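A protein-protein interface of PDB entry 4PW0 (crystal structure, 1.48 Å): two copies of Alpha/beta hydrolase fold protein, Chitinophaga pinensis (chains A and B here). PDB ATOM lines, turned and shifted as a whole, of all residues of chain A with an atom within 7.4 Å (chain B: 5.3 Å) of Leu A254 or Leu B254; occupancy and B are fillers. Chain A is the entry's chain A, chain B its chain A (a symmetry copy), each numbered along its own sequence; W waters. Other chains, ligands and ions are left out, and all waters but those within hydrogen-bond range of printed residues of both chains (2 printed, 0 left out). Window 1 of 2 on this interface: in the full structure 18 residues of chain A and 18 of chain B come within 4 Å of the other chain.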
ATOM      1  N   ILE A 132      19.918  15.101 -25.414  1.00  0.00           N
ATOM      2  CA  ILE A 132      21.060  15.224 -26.307  1.00  0.00           C
ATOM      3  C   ILE A 132      21.669  16.596 -26.056  1.00  0.00           C
ATOM      4  O   ILE A 132      20.978  17.603 -26.216  1.00  0.00           O
ATOM      5  CB  ILE A 132      20.680  15.079 -27.788  1.00  0.00           C
ATOM      6  CG1 ILE A 132      20.088  13.716 -28.061  1.00  0.00           C
ATOM      7  CG2 ILE A 132      21.892  15.370 -28.678  1.00  0.00           C
ATOM      8  CD1 ILE A 132      19.480  13.571 -29.433  1.00  0.00           C
ATOM      9  N   VAL A 226      12.366  13.925 -26.630  1.00  0.00           N
ATOM     10  CA  VAL A 226      13.778  14.293 -26.657  1.00  0.00           C
ATOM     11  C   VAL A 226      13.917  15.723 -26.187  1.00  0.00           C
ATOM     12  O   VAL A 226      13.107  16.596 -26.556  1.00  0.00           O
ATOM     13  CB  VAL A 226      14.384  14.159 -28.080  1.00  0.00           C
ATOM     14  CG1 VAL A 226      15.887  14.445 -28.069  1.00  0.00           C
ATOM     15  CG2 VAL A 226      14.141  12.756 -28.632  1.00  0.00           C
ATOM     16  N   PHE A 227      14.990  15.993 -25.442  1.00  0.00           N
ATOM     17  CA  PHE A 227      15.338  17.356 -25.066  1.00  0.00           C
ATOM     18  C   PHE A 227      16.732  17.619 -25.622  1.00  0.00           C
ATOM     19  O   PHE A 227      17.693  16.904 -25.254  1.00  0.00           O
ATOM     20  CB  PHE A 227      15.330  17.459 -23.558  1.00  0.00           C
ATOM     21  CG  PHE A 227      15.746  18.789 -23.011  1.00  0.00           C
ATOM     22  CD1 PHE A 227      15.436  19.976 -23.684  1.00  0.00           C
ATOM     23  CD2 PHE A 227      16.432  18.860 -21.823  1.00  0.00           C
ATOM     24  CE1 PHE A 227      15.766  21.213 -23.142  1.00  0.00           C
ATOM     25  CE2 PHE A 227      16.755  20.088 -21.271  1.00  0.00           C
ATOM     26  CZ  PHE A 227      16.462  21.255 -21.946  1.00  0.00           C
ATOM     27  N   VAL A 228      16.844  18.593 -26.526  1.00  0.00           N
ATOM     28  CA  VAL A 228      18.102  18.882 -27.235  1.00  0.00           C
ATOM     29  C   VAL A 228      18.605  20.219 -26.674  1.00  0.00           C
ATOM     30  O   VAL A 228      17.883  21.212 -26.720  1.00  0.00           O
ATOM     31  CB  VAL A 228      17.880  19.013 -28.744  1.00  0.00           C
ATOM     32  CG1 VAL A 228      19.178  19.351 -29.433  1.00  0.00           C
ATOM     33  CG2 VAL A 228      17.265  17.754 -29.364  1.00  0.00           C
ATOM     34  N   VAL A 229      19.854  20.225 -26.207  1.00  0.00           N
ATOM     35  CA  VAL A 229      20.487  21.432 -25.646  1.00  0.00           C
ATOM     36  C   VAL A 229      21.767  21.741 -26.432  1.00  0.00           C
ATOM     37  O   VAL A 229      22.573  20.851 -26.771  1.00  0.00           O
ATOM     38  CB  VAL A 229      20.838  21.219 -24.165  1.00  0.00           C
ATOM     39  CG1 VAL A 229      21.658  22.375 -23.591  1.00  0.00           C
ATOM     40  CG2 VAL A 229      19.576  20.999 -23.353  1.00  0.00           C
ATOM     41  N   GLN A 230      21.961  23.023 -26.720  1.00  0.00           N
ATOM     42  CA  GLN A 230      23.152  23.472 -27.441  1.00  0.00           C
ATOM     43  C   GLN A 230      23.429  24.935 -27.109  1.00  0.00           C
ATOM     44  O   GLN A 230      22.526  25.651 -26.663  1.00  0.00           O
ATOM     45  CB  GLN A 230      22.911  23.226 -28.934  1.00  0.00           C
ATOM     46  CG  GLN A 230      24.029  23.573 -29.903  1.00  0.00           C
ATOM     47  CD  GLN A 230      25.335  22.910 -29.546  1.00  0.00           C
ATOM     48  OE1 GLN A 230      25.985  23.317 -28.568  1.00  0.00           O
ATOM     49  NE2 GLN A 230      25.770  21.933 -30.315  1.00  0.00           N
ATOM     50  N   THR A 239      25.940  24.697 -34.255  1.00  0.00           N
ATOM     51  CA  THR A 239      24.701  24.917 -33.554  1.00  0.00           C
ATOM     52  C   THR A 239      23.488  24.628 -34.429  1.00  0.00           C
ATOM     53  O   THR A 239      22.488  24.107 -33.930  1.00  0.00           O
ATOM     54  CB  THR A 239      24.689  26.316 -32.982  1.00  0.00           C
ATOM     55  OG1 THR A 239      25.685  26.370 -31.950  1.00  0.00           O
ATOM     56  CG2 THR A 239      23.324  26.712 -32.415  1.00  0.00           C
ATOM     57  N   TYR A 240      23.547  24.968 -35.722  1.00  0.00           N
ATOM     58  CA  TYR A 240      22.378  24.747 -36.566  1.00  0.00           C
ATOM     59  C   TYR A 240      21.979  23.303 -36.660  1.00  0.00           C
ATOM     60  O   TYR A 240      20.801  22.971 -36.846  1.00  0.00           O
ATOM     61  CB  TYR A 240      22.625  25.324 -37.967  1.00  0.00           C
ATOM     62  CG  TYR A 240      21.370  25.352 -38.795  1.00  0.00           C
ATOM     63  CD1 TYR A 240      20.448  26.327 -38.640  1.00  0.00           C
ATOM     64  CD2 TYR A 240      21.123  24.337 -39.668  1.00  0.00           C
ATOM     65  CE1 TYR A 240      19.273  26.331 -39.372  1.00  0.00           C
ATOM     66  CE2 TYR A 240      19.940  24.294 -40.408  1.00  0.00           C
ATOM     67  CZ  TYR A 240      19.036  25.310 -40.262  1.00  0.00           C
ATOM     68  OH  TYR A 240      17.850  25.322 -40.971  1.00  0.00           O
ATOM     69  N   ASN A 241      22.935  22.405 -36.474  1.00  0.00           N
ATOM     70  CA  ASN A 241      22.601  20.976 -36.466  1.00  0.00           C
ATOM     71  C   ASN A 241      21.712  20.535 -35.297  1.00  0.00           C
ATOM     72  O   ASN A 241      21.060  19.480 -35.377  1.00  0.00           O
ATOM     73  CB  ASN A 241      23.836  20.111 -36.585  1.00  0.00           C
ATOM     74  CG  ASN A 241      24.394  20.151 -37.979  1.00  0.00           C
ATOM     75  OD1 ASN A 241      23.627  20.178 -38.967  1.00  0.00           O
ATOM     76  ND2 ASN A 241      25.705  20.119 -38.087  1.00  0.00           N
ATOM     77  N   SER A 242      21.661  21.336 -34.230  1.00  0.00           N
ATOM     78  CA  SER A 242      20.718  21.077 -33.160  1.00  0.00           C
ATOM     79  C   SER A 242      19.318  21.550 -33.546  1.00  0.00           C
ATOM     80  O   SER A 242      18.307  20.909 -33.162  1.00  0.00           O
ATOM     81  CB  SER A 242      21.193  21.699 -31.854  1.00  0.00           C
ATOM     82  OG  SER A 242      22.324  20.981 -31.350  1.00  0.00           O
ATOM     83  N   TYR A 243      19.243  22.656 -34.268  1.00  0.00           N
ATOM     84  CA  TYR A 243      17.978  23.037 -34.898  1.00  0.00           C
ATOM     85  C   TYR A 243      17.517  21.960 -35.879  1.00  0.00           C
ATOM     86  O   TYR A 243      16.333  21.604 -35.917  1.00  0.00           O
ATOM     87  CB  TYR A 243      18.066  24.419 -35.539  1.00  0.00           C
ATOM     88  CG  TYR A 243      16.759  24.947 -36.100  1.00  0.00           C
ATOM     89  CD1 TYR A 243      15.625  24.938 -35.361  1.00  0.00           C
ATOM     90  CD2 TYR A 243      16.671  25.391 -37.403  1.00  0.00           C
ATOM     91  CE1 TYR A 243      14.449  25.399 -35.841  1.00  0.00           C
ATOM     92  CE2 TYR A 243      15.472  25.828 -37.912  1.00  0.00           C
ATOM     93  CZ  TYR A 243      14.368  25.849 -37.076  1.00  0.00           C
ATOM     94  OH  TYR A 243      13.167  26.327 -37.495  1.00  0.00           O
ATOM     95  N   GLU A 244      18.443  21.370 -36.640  1.00  0.00           N
ATOM     96  CA  GLU A 244      18.088  20.252 -37.515  1.00  0.00           C
ATOM     97  C   GLU A 244      17.532  19.065 -36.757  1.00  0.00           C
ATOM     98  O   GLU A 244      16.527  18.465 -37.174  1.00  0.00           O
ATOM     99  CB  GLU A 244      19.281  19.765 -38.359  1.00  0.00           C
ATOM    100  CG  GLU A 244      19.603  20.683 -39.517  1.00  0.00           C
ATOM    101  CD  GLU A 244      18.614  20.556 -40.673  1.00  0.00           C
ATOM    102  OE1 GLU A 244      17.649  19.746 -40.560  1.00  0.00           O
ATOM    103  OE2 GLU A 244      18.815  21.248 -41.692  1.00  0.00           O
ATOM    104  N   LEU A 245      18.147  18.705 -35.632  1.00  0.00           N
ATOM    105  CA  LEU A 245      17.592  17.651 -34.784  1.00  0.00           C
ATOM    106  C   LEU A 245      16.162  17.984 -34.395  1.00  0.00           C
ATOM    107  O   LEU A 245      15.255  17.128 -34.460  1.00  0.00           O
ATOM    108  CB  LEU A 245      18.446  17.373 -33.524  1.00  0.00           C
ATOM    109  CG  LEU A 245      19.740  16.580 -33.725  1.00  0.00           C
ATOM    110  CD1 LEU A 245      20.613  16.707 -32.512  1.00  0.00           C
ATOM    111  CD2 LEU A 245      19.438  15.108 -34.018  1.00  0.00           C
ATOM    112  N   PHE A 246      15.939  19.199 -33.944  1.00  0.00           N
ATOM    113  CA  PHE A 246      14.612  19.643 -33.513  1.00  0.00           C
ATOM    114  C   PHE A 246      13.600  19.568 -34.677  1.00  0.00           C
ATOM    115  O   PHE A 246      12.451  19.112 -34.488  1.00  0.00           O
ATOM    116  CB  PHE A 246      14.679  21.094 -33.012  1.00  0.00           C
ATOM    117  CG  PHE A 246      13.328  21.723 -32.778  1.00  0.00           C
ATOM    118  CD1 PHE A 246      12.587  21.441 -31.637  1.00  0.00           C
ATOM    119  CD2 PHE A 246      12.796  22.573 -33.730  1.00  0.00           C
ATOM    120  CE1 PHE A 246      11.318  21.967 -31.475  1.00  0.00           C
ATOM    121  CE2 PHE A 246      11.536  23.095 -33.564  1.00  0.00           C
ATOM    122  CZ  PHE A 246      10.801  22.793 -32.418  1.00  0.00           C
ATOM    123  N   LYS A 247      14.018  19.985 -35.881  1.00  0.00           N
ATOM    124  CA  LYS A 247      13.128  19.937 -37.044  1.00  0.00           C
ATOM    125  C   LYS A 247      12.753  18.517 -37.434  1.00  0.00           C
ATOM    126  O   LYS A 247      11.601  18.260 -37.793  1.00  0.00           O
ATOM    127  CB  LYS A 247      13.771  20.606 -38.248  1.00  0.00           C
ATOM    128  CG  LYS A 247      13.858  22.094 -38.097  1.00  0.00           C
ATOM    129  CD  LYS A 247      14.118  22.793 -39.407  1.00  0.00           C
ATOM    130  CE  LYS A 247      15.440  22.559 -39.955  1.00  0.00           C
ATOM    131  NZ  LYS A 247      15.478  23.268 -41.274  1.00  0.00           N
ATOM    132  N   ALA A 252      10.725  16.602 -30.047  1.00  0.00           N
ATOM    133  CA  ALA A 252      11.882  17.216 -29.374  1.00  0.00           C
ATOM    134  C   ALA A 252      11.588  18.641 -28.937  1.00  0.00           C
ATOM    135  O   ALA A 252      11.039  19.456 -29.700  1.00  0.00           O
ATOM    136  CB  ALA A 252      13.139  17.216 -30.258  1.00  0.00           C
ATOM    137  N   ILE A 253      12.026  18.934 -27.711  1.00  0.00           N
ATOM    138  CA  ILE A 253      12.130  20.315 -27.234  1.00  0.00           C
ATOM    139  C   ILE A 253      13.580  20.767 -27.473  1.00  0.00           C
ATOM    140  O   ILE A 253      14.515  20.015 -27.210  1.00  0.00           O
ATOM    141  CB  ILE A 253      11.825  20.399 -25.719  1.00  0.00           C
ATOM    142  CG1 ILE A 253      10.423  19.948 -25.383  1.00  0.00           C
ATOM    143  CG2 ILE A 253      12.141  21.774 -25.170  1.00  0.00           C
ATOM    144  CD1 ILE A 253      10.248  19.490 -23.950  1.00  0.00           C
ATOM    145  N   LEU A 254      13.761  21.977 -27.993  1.00  0.00           N
ATOM    146  CA  LEU A 254      15.101  22.539 -28.149  1.00  0.00           C
ATOM    147  C   LEU A 254      15.310  23.645 -27.137  1.00  0.00           C
ATOM    148  O   LEU A 254      14.408  24.491 -26.948  1.00  0.00           O
ATOM    149  CB  LEU A 254      15.259  23.177 -29.544  1.00  0.00           C
ATOM    150  CG  LEU A 254      16.604  23.765 -29.898  1.00  0.00           C
ATOM    151  CD1 LEU A 254      17.696  22.723 -29.940  1.00  0.00           C
ATOM    152  CD2 LEU A 254      16.517  24.503 -31.229  1.00  0.00           C
ATOM    153  N   SER A 255      16.500  23.716 -26.555  1.00  0.00           N
ATOM    154  CA  SER A 255      16.980  24.877 -25.790  1.00  0.00           C
ATOM    155  C   SER A 255      18.334  25.309 -26.339  1.00  0.00           C
ATOM    156  O   SER A 255      19.242  24.479 -26.432  1.00  0.00           O
ATOM    157  CB  SER A 255      17.172  24.476 -24.304  1.00  0.00           C
ATOM    158  OG  SER A 255      15.959  24.360 -23.537  1.00  0.00           O
ATOM    159  N   LEU A 256      18.458  26.586 -26.696  1.00  0.00           N
ATOM    160  CA  LEU A 256      19.750  27.150 -27.048  1.00  0.00           C
ATOM    161  C   LEU A 256      20.152  28.200 -26.011  1.00  0.00           C
ATOM    162  O   LEU A 256      19.346  29.053 -25.602  1.00  0.00           O
ATOM    163  CB  LEU A 256      19.757  27.792 -28.429  1.00  0.00           C
ATOM    164  CG  LEU A 256      19.370  26.920 -29.602  1.00  0.00           C
ATOM    165  CD1 LEU A 256      19.466  27.705 -30.897  1.00  0.00           C
ATOM    166  CD2 LEU A 256      20.213  25.674 -29.649  1.00  0.00           C
ATOM    167  N   TYR A 257      21.416  28.102 -25.594  1.00  0.00           N
ATOM    168  CA  TYR A 257      21.951  28.943 -24.514  1.00  0.00           C
ATOM    169  C   TYR A 257      22.878  30.051 -25.050  1.00  0.00           C
ATOM    170  O   TYR A 257      23.643  29.803 -25.978  1.00  0.00           O
ATOM    171  CB  TYR A 257      22.704  28.102 -23.462  1.00  0.00           C
ATOM    172  CG  TYR A 257      21.895  27.044 -22.737  1.00  0.00           C
ATOM    173  CD1 TYR A 257      20.516  27.019 -22.746  1.00  0.00           C
ATOM    174  CD2 TYR A 257      22.554  26.087 -21.960  1.00  0.00           C
ATOM    175  CE1 TYR A 257      19.777  26.060 -22.040  1.00  0.00           C
ATOM    176  CE2 TYR A 257      21.839  25.139 -21.279  1.00  0.00           C
ATOM    177  CZ  TYR A 257      20.494  25.103 -21.310  1.00  0.00           C
ATOM    178  OH  TYR A 257      19.814  24.115 -20.594  1.00  0.00           O
ATOM    179  N   PRO A 258      22.795  31.242 -24.463  1.00  0.00           N
ATOM    180  CA  PRO A 258      23.475  32.406 -25.081  1.00  0.00           C
ATOM    181  C   PRO A 258      24.965  32.446 -24.857  1.00  0.00           C
ATOM    182  O   PRO A 258      25.481  32.046 -23.790  1.00  0.00           O
ATOM    183  CB  PRO A 258      22.809  33.582 -24.372  1.00  0.00           C
ATOM    184  CG  PRO A 258      22.339  33.031 -23.047  1.00  0.00           C
ATOM    185  CD  PRO A 258      21.886  31.623 -23.377  1.00  0.00           C
ATOM    186  N   GLN A 275      15.922  22.746 -16.410  1.00  0.00           N
ATOM    187  CA  GLN A 275      15.184  22.335 -17.612  1.00  0.00           C
ATOM    188  C   GLN A 275      15.034  20.832 -17.728  1.00  0.00           C
ATOM    189  O   GLN A 275      13.930  20.332 -18.078  1.00  0.00           O
ATOM    190  CB  GLN A 275      15.864  22.896 -18.851  1.00  0.00           C
ATOM    191  CG  GLN A 275      15.780  24.382 -18.941  1.00  0.00           C
ATOM    192  CD  GLN A 275      16.258  24.896 -20.273  1.00  0.00           C
ATOM    193  OE1 GLN A 275      17.069  24.287 -20.928  1.00  0.00           O
ATOM    194  NE2 GLN A 275      15.746  26.101 -20.635  1.00  0.00           N
ATOM    195  N   PHE B 227      14.192  35.670 -22.671  1.00  0.00           N
ATOM    196  CA  PHE B 227      13.805  34.282 -22.880  1.00  0.00           C
ATOM    197  C   PHE B 227      12.812  34.277 -24.035  1.00  0.00           C
ATOM    198  O   PHE B 227      11.741  34.922 -23.938  1.00  0.00           O
ATOM    199  CB  PHE B 227      13.164  33.762 -21.615  1.00  0.00           C
ATOM    200  CG  PHE B 227      12.640  32.362 -21.698  1.00  0.00           C
ATOM    201  CD1 PHE B 227      13.288  31.393 -22.471  1.00  0.00           C
ATOM    202  CD2 PHE B 227      11.512  32.008 -20.998  1.00  0.00           C
ATOM    203  CE1 PHE B 227      12.837  30.079 -22.495  1.00  0.00           C
ATOM    204  CE2 PHE B 227      11.063  30.698 -21.008  1.00  0.00           C
ATOM    205  CZ  PHE B 227      11.695  29.749 -21.784  1.00  0.00           C
ATOM    206  N   VAL B 228      13.167  33.603 -25.131  1.00  0.00           N
ATOM    207  CA  VAL B 228      12.364  33.606 -26.364  1.00  0.00           C
ATOM    208  C   VAL B 228      11.755  32.201 -26.476  1.00  0.00           C
ATOM    209  O   VAL B 228      12.489  31.216 -26.479  1.00  0.00           O
ATOM    210  CB  VAL B 228      13.227  33.887 -27.597  1.00  0.00           C
ATOM    211  CG1 VAL B 228      12.382  33.840 -28.845  1.00  0.00           C
ATOM    212  CG2 VAL B 228      13.966  35.226 -27.509  1.00  0.00           C
ATOM    213  N   VAL B 229      10.431  32.146 -26.620  1.00  0.00           N
ATOM    214  CA  VAL B 229       9.697  30.875 -26.751  1.00  0.00           C
ATOM    215  C   VAL B 229       8.909  30.882 -28.067  1.00  0.00           C
ATOM    216  O   VAL B 229       8.274  31.882 -28.458  1.00  0.00           O
ATOM    217  CB  VAL B 229       8.724  30.689 -25.575  1.00  0.00           C
ATOM    218  CG1 VAL B 229       7.814  29.475 -25.763  1.00  0.00           C
ATOM    219  CG2 VAL B 229       9.492  30.591 -24.271  1.00  0.00           C
ATOM    220  N   SER B 242      12.365  33.439 -34.586  1.00  0.00           N
ATOM    221  CA  SER B 242      12.730  33.327 -33.188  1.00  0.00           C
ATOM    222  C   SER B 242      14.186  32.890 -33.042  1.00  0.00           C
ATOM    223  O   SER B 242      14.886  33.331 -32.095  1.00  0.00           O
ATOM    224  CB  SER B 242      11.777  32.398 -32.449  1.00  0.00           C
ATOM    225  OG  SER B 242      10.495  33.019 -32.308  1.00  0.00           O
ATOM    226  N   TYR B 243      14.640  32.027 -33.937  1.00  0.00           N
ATOM    227  CA  TYR B 243      16.075  31.755 -34.033  1.00  0.00           C
ATOM    228  C   TYR B 243      16.845  33.031 -34.372  1.00  0.00           C
ATOM    229  O   TYR B 243      17.901  33.305 -33.791  1.00  0.00           O
ATOM    230  CB  TYR B 243      16.364  30.616 -35.006  1.00  0.00           C
ATOM    231  CG  TYR B 243      17.816  30.181 -35.067  1.00  0.00           C
ATOM    232  CD1 TYR B 243      18.514  29.909 -33.938  1.00  0.00           C
ATOM    233  CD2 TYR B 243      18.490  30.113 -36.267  1.00  0.00           C
ATOM    234  CE1 TYR B 243      19.809  29.525 -33.967  1.00  0.00           C
ATOM    235  CE2 TYR B 243      19.817  29.758 -36.305  1.00  0.00           C
ATOM    236  CZ  TYR B 243      20.447  29.433 -35.115  1.00  0.00           C
ATOM    237  OH  TYR B 243      21.739  29.014 -35.086  1.00  0.00           O
ATOM    238  N   PHE B 246      17.242  35.033 -31.259  1.00  0.00           N
ATOM    239  CA  PHE B 246      18.275  34.401 -30.438  1.00  0.00           C
ATOM    240  C   PHE B 246      19.685  34.732 -30.975  1.00  0.00           C
ATOM    241  O   PHE B 246      20.606  35.040 -30.187  1.00  0.00           O
ATOM    242  CB  PHE B 246      18.092  32.875 -30.443  1.00  0.00           C
ATOM    243  CG  PHE B 246      19.245  32.119 -29.831  1.00  0.00           C
ATOM    244  CD1 PHE B 246      19.398  32.022 -28.454  1.00  0.00           C
ATOM    245  CD2 PHE B 246      20.192  31.535 -30.653  1.00  0.00           C
ATOM    246  CE1 PHE B 246      20.502  31.390 -27.910  1.00  0.00           C
ATOM    247  CE2 PHE B 246      21.286  30.907 -30.109  1.00  0.00           C
ATOM    248  CZ  PHE B 246      21.429  30.829 -28.723  1.00  0.00           C
ATOM    249  N   ALA B 252      20.063  36.093 -24.932  1.00  0.00           N
ATOM    250  CA  ALA B 252      18.772  35.393 -25.030  1.00  0.00           C
ATOM    251  C   ALA B 252      18.939  33.887 -24.926  1.00  0.00           C
ATOM    252  O   ALA B 252      19.817  33.283 -25.568  1.00  0.00           O
ATOM    253  CB  ALA B 252      18.027  35.722 -26.333  1.00  0.00           C
ATOM    254  N   ILE B 253      18.032  33.292 -24.148  1.00  0.00           N
ATOM    255  CA  ILE B 253      17.822  31.843 -24.170  1.00  0.00           C
ATOM    256  C   ILE B 253      16.653  31.572 -25.130  1.00  0.00           C
ATOM    257  O   ILE B 253      15.649  32.279 -25.102  1.00  0.00           O
ATOM    258  CB  ILE B 253      17.444  31.320 -22.763  1.00  0.00           C
ATOM    259  CG1 ILE B 253      18.528  31.567 -21.740  1.00  0.00           C
ATOM    260  CG2 ILE B 253      17.010  29.870 -22.814  1.00  0.00           C
ATOM    261  CD1 ILE B 253      18.032  31.594 -20.310  1.00  0.00           C
ATOM    262  N   LEU B 254      16.795  30.569 -25.992  1.00  0.00           N
ATOM    263  CA  LEU B 254      15.695  30.161 -26.865  1.00  0.00           C
ATOM    264  C   LEU B 254      15.141  28.833 -26.397  1.00  0.00           C
ATOM    265  O   LEU B 254      15.924  27.911 -26.079  1.00  0.00           O
ATOM    266  CB  LEU B 254      16.201  29.950 -28.306  1.00  0.00           C
ATOM    267  CG  LEU B 254      15.185  29.573 -29.357  1.00  0.00           C
ATOM    268  CD1 LEU B 254      14.154  30.654 -29.577  1.00  0.00           C
ATOM    269  CD2 LEU B 254      15.889  29.231 -30.665  1.00  0.00           C
ATOM    270  N   SER B 255      13.823  28.680 -26.435  1.00  0.00           N
ATOM    271  CA  SER B 255      13.135  27.386 -26.312  1.00  0.00           C
ATOM    272  C   SER B 255      12.186  27.214 -27.491  1.00  0.00           C
ATOM    273  O   SER B 255      11.356  28.094 -27.734  1.00  0.00           O
ATOM    274  CB  SER B 255      12.291  27.368 -25.011  1.00  0.00           C
ATOM    275  OG  SER B 255      13.040  27.186 -23.796  1.00  0.00           O
ATOM    276  N   LEU B 256      12.313  26.097 -28.208  1.00  0.00           N
ATOM    277  CA  LEU B 256      11.341  25.740 -29.227  1.00  0.00           C
ATOM    278  C   LEU B 256      10.598  24.471 -28.806  1.00  0.00           C
ATOM    279  O   LEU B 256      11.201  23.487 -28.344  1.00  0.00           O
ATOM    280  CB  LEU B 256      11.977  25.510 -30.592  1.00  0.00           C
ATOM    281  CG  LEU B 256      12.777  26.648 -31.185  1.00  0.00           C
ATOM    282  CD1 LEU B 256      13.304  26.264 -32.555  1.00  0.00           C
ATOM    283  CD2 LEU B 256      11.959  27.910 -31.244  1.00  0.00           C
ATOM    284  N   TYR B 257       9.276  24.531 -28.971  1.00  0.00           N
ATOM    285  CA  TYR B 257       8.381  23.459 -28.513  1.00  0.00           C
ATOM    286  C   TYR B 257       7.853  22.608 -29.684  1.00  0.00           C
ATOM    287  O   TYR B 257       7.552  23.154 -30.741  1.00  0.00           O
ATOM    288  CB  TYR B 257       7.192  24.020 -27.704  1.00  0.00           C
ATOM    289  CG  TYR B 257       7.535  24.779 -26.437  1.00  0.00           C
ATOM    290  CD1 TYR B 257       8.776  24.715 -25.839  1.00  0.00           C
ATOM    291  CD2 TYR B 257       6.544  25.522 -25.791  1.00  0.00           C
ATOM    292  CE1 TYR B 257       9.071  25.388 -24.646  1.00  0.00           C
ATOM    293  CE2 TYR B 257       6.828  26.193 -24.632  1.00  0.00           C
ATOM    294  CZ  TYR B 257       8.048  26.148 -24.065  1.00  0.00           C
ATOM    295  OH  TYR B 257       8.283  26.851 -22.881  1.00  0.00           O
HETATM  296  O   HOH W   1      13.312  24.575 -24.123  1.00  0.00           O
HETATM  297  O   HOH W   2      15.687  26.970 -23.208  1.00  0.00           O
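Of the 12 printed residues of chain B, 8 touch a printed residue of chain A.
Among the printed residues, no Asp or Glu carboxylate lies within 4 Å of a Lys or Arg side-chain nitrogen of the other chain.
Tyr A243 touches Leu B256, and with the chains exchanged Leu A256 touches Tyr B243.
Phe A246 touches Leu B256, and with the chains exchanged Leu A256 touches Phe B246.
Ile A253 touches Leu B256, and with the chains exchanged Leu A256 touches Ile B253.
Leu A254 touches Leu B256, and with the chains exchanged Leu A256 touches Leu B254.
12 positions are printed for both chains.
Of the 16 pairs that touch across the chains among the printed residues, 13 have their exchanged pair printed and touching as well.
N of Val A228 is in hydrogen-bond range of O of Ile A253 (2.8 Å).
O of Gln A230 sits at hydrogen-bond distance from N of Tyr A257, at 2.9 Å.
OG of Ser A255 sits at hydrogen-bond distance from OE1 of Gln A275 (2.8 Å).
The side-chain hydroxyl (OH) of Tyr A257 lies within hydrogen-bond range of the side-chain amide oxygen (OE1) of Gln A275, at 2.8 Å.
N of Val B228 lies within hydrogen-bond range of O of Ile B253 (2.8 Å).
The backbone NH (N) of Ser B255 lies within hydrogen-bond range of the backbone carbonyl oxygen (O) of Val B228 (2.9 Å).
Water W1 lies within hydrogen-bond range of OG of Ser B255 (2.6 Å), OG of Ser A255 (2.7 Å) and O of Leu A254 (3.0 Å).
Water W2 lies within hydrogen-bond range of OG of Ser A255, NE2 of Gln A275, OG of Ser B255 and O of Leu B254.
OH of Tyr B243 touches CG2 of Thr A239 (3.9 Å).
CZ of Phe A246 touches CB of Leu B256, at 3.5 Å.
Tyr B257 touches Phe A246.
Ile A253 touches Leu B256 (CA to O, 3.5 Å).
Ser B255 touches Leu A254.
Leu A256 touches Tyr B243.
Leu A256 touches Ile B253.
Tyr A257 touches Phe B246 (O to CZ, 3.7 Å).
CB of Pro A258 touches O of Ala B252 (3.2 Å).
Ile B253 touches Pro A258.
The backbone carbonyl oxygen of Leu A254 is in hydrogen-bond range of the backbone NH of Leu B256, 2.9 Å away.
The backbone NH (N) of Leu A256 sits at hydrogen-bond distance from the backbone carbonyl oxygen (O) of Leu B254, 2.9 Å away.
Gln A230 touches none of the printed residues of chain B.
Of the printed residues of chain B, Leu A254 touches Leu B254 (3.8 Å), Ser B255 (3.2 Å) and Leu B256 (2.9 Å).
Printed residues of chain B within 4 Å of Ser A255: Leu B254 (3.2 Å).
Of the printed residues of chain B, Tyr A257 touches Phe B246.
Printed residues of chain A within 4 Å of Tyr B243: Thr A239 (3.9 Å) and Leu A256 (3.6 Å).
Printed residues of chain A within 4 Å of Leu B254: Leu A254 (3.8 Å), Ser A255 (3.2 Å) and Leu A256 (2.9 Å).
Of the printed residues of chain A, Ser B255 touches Leu A254 (3.2 Å).
Printed residues of chain A within 4 Å of Tyr B257: Phe A246.
The nearest printed residue of chain A that does not touch Leu B254 is Tyr A257 (5.3 Å).
The nearest printed residue of chain A that does not touch Tyr B257 is Ala A252 (4.5 Å).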
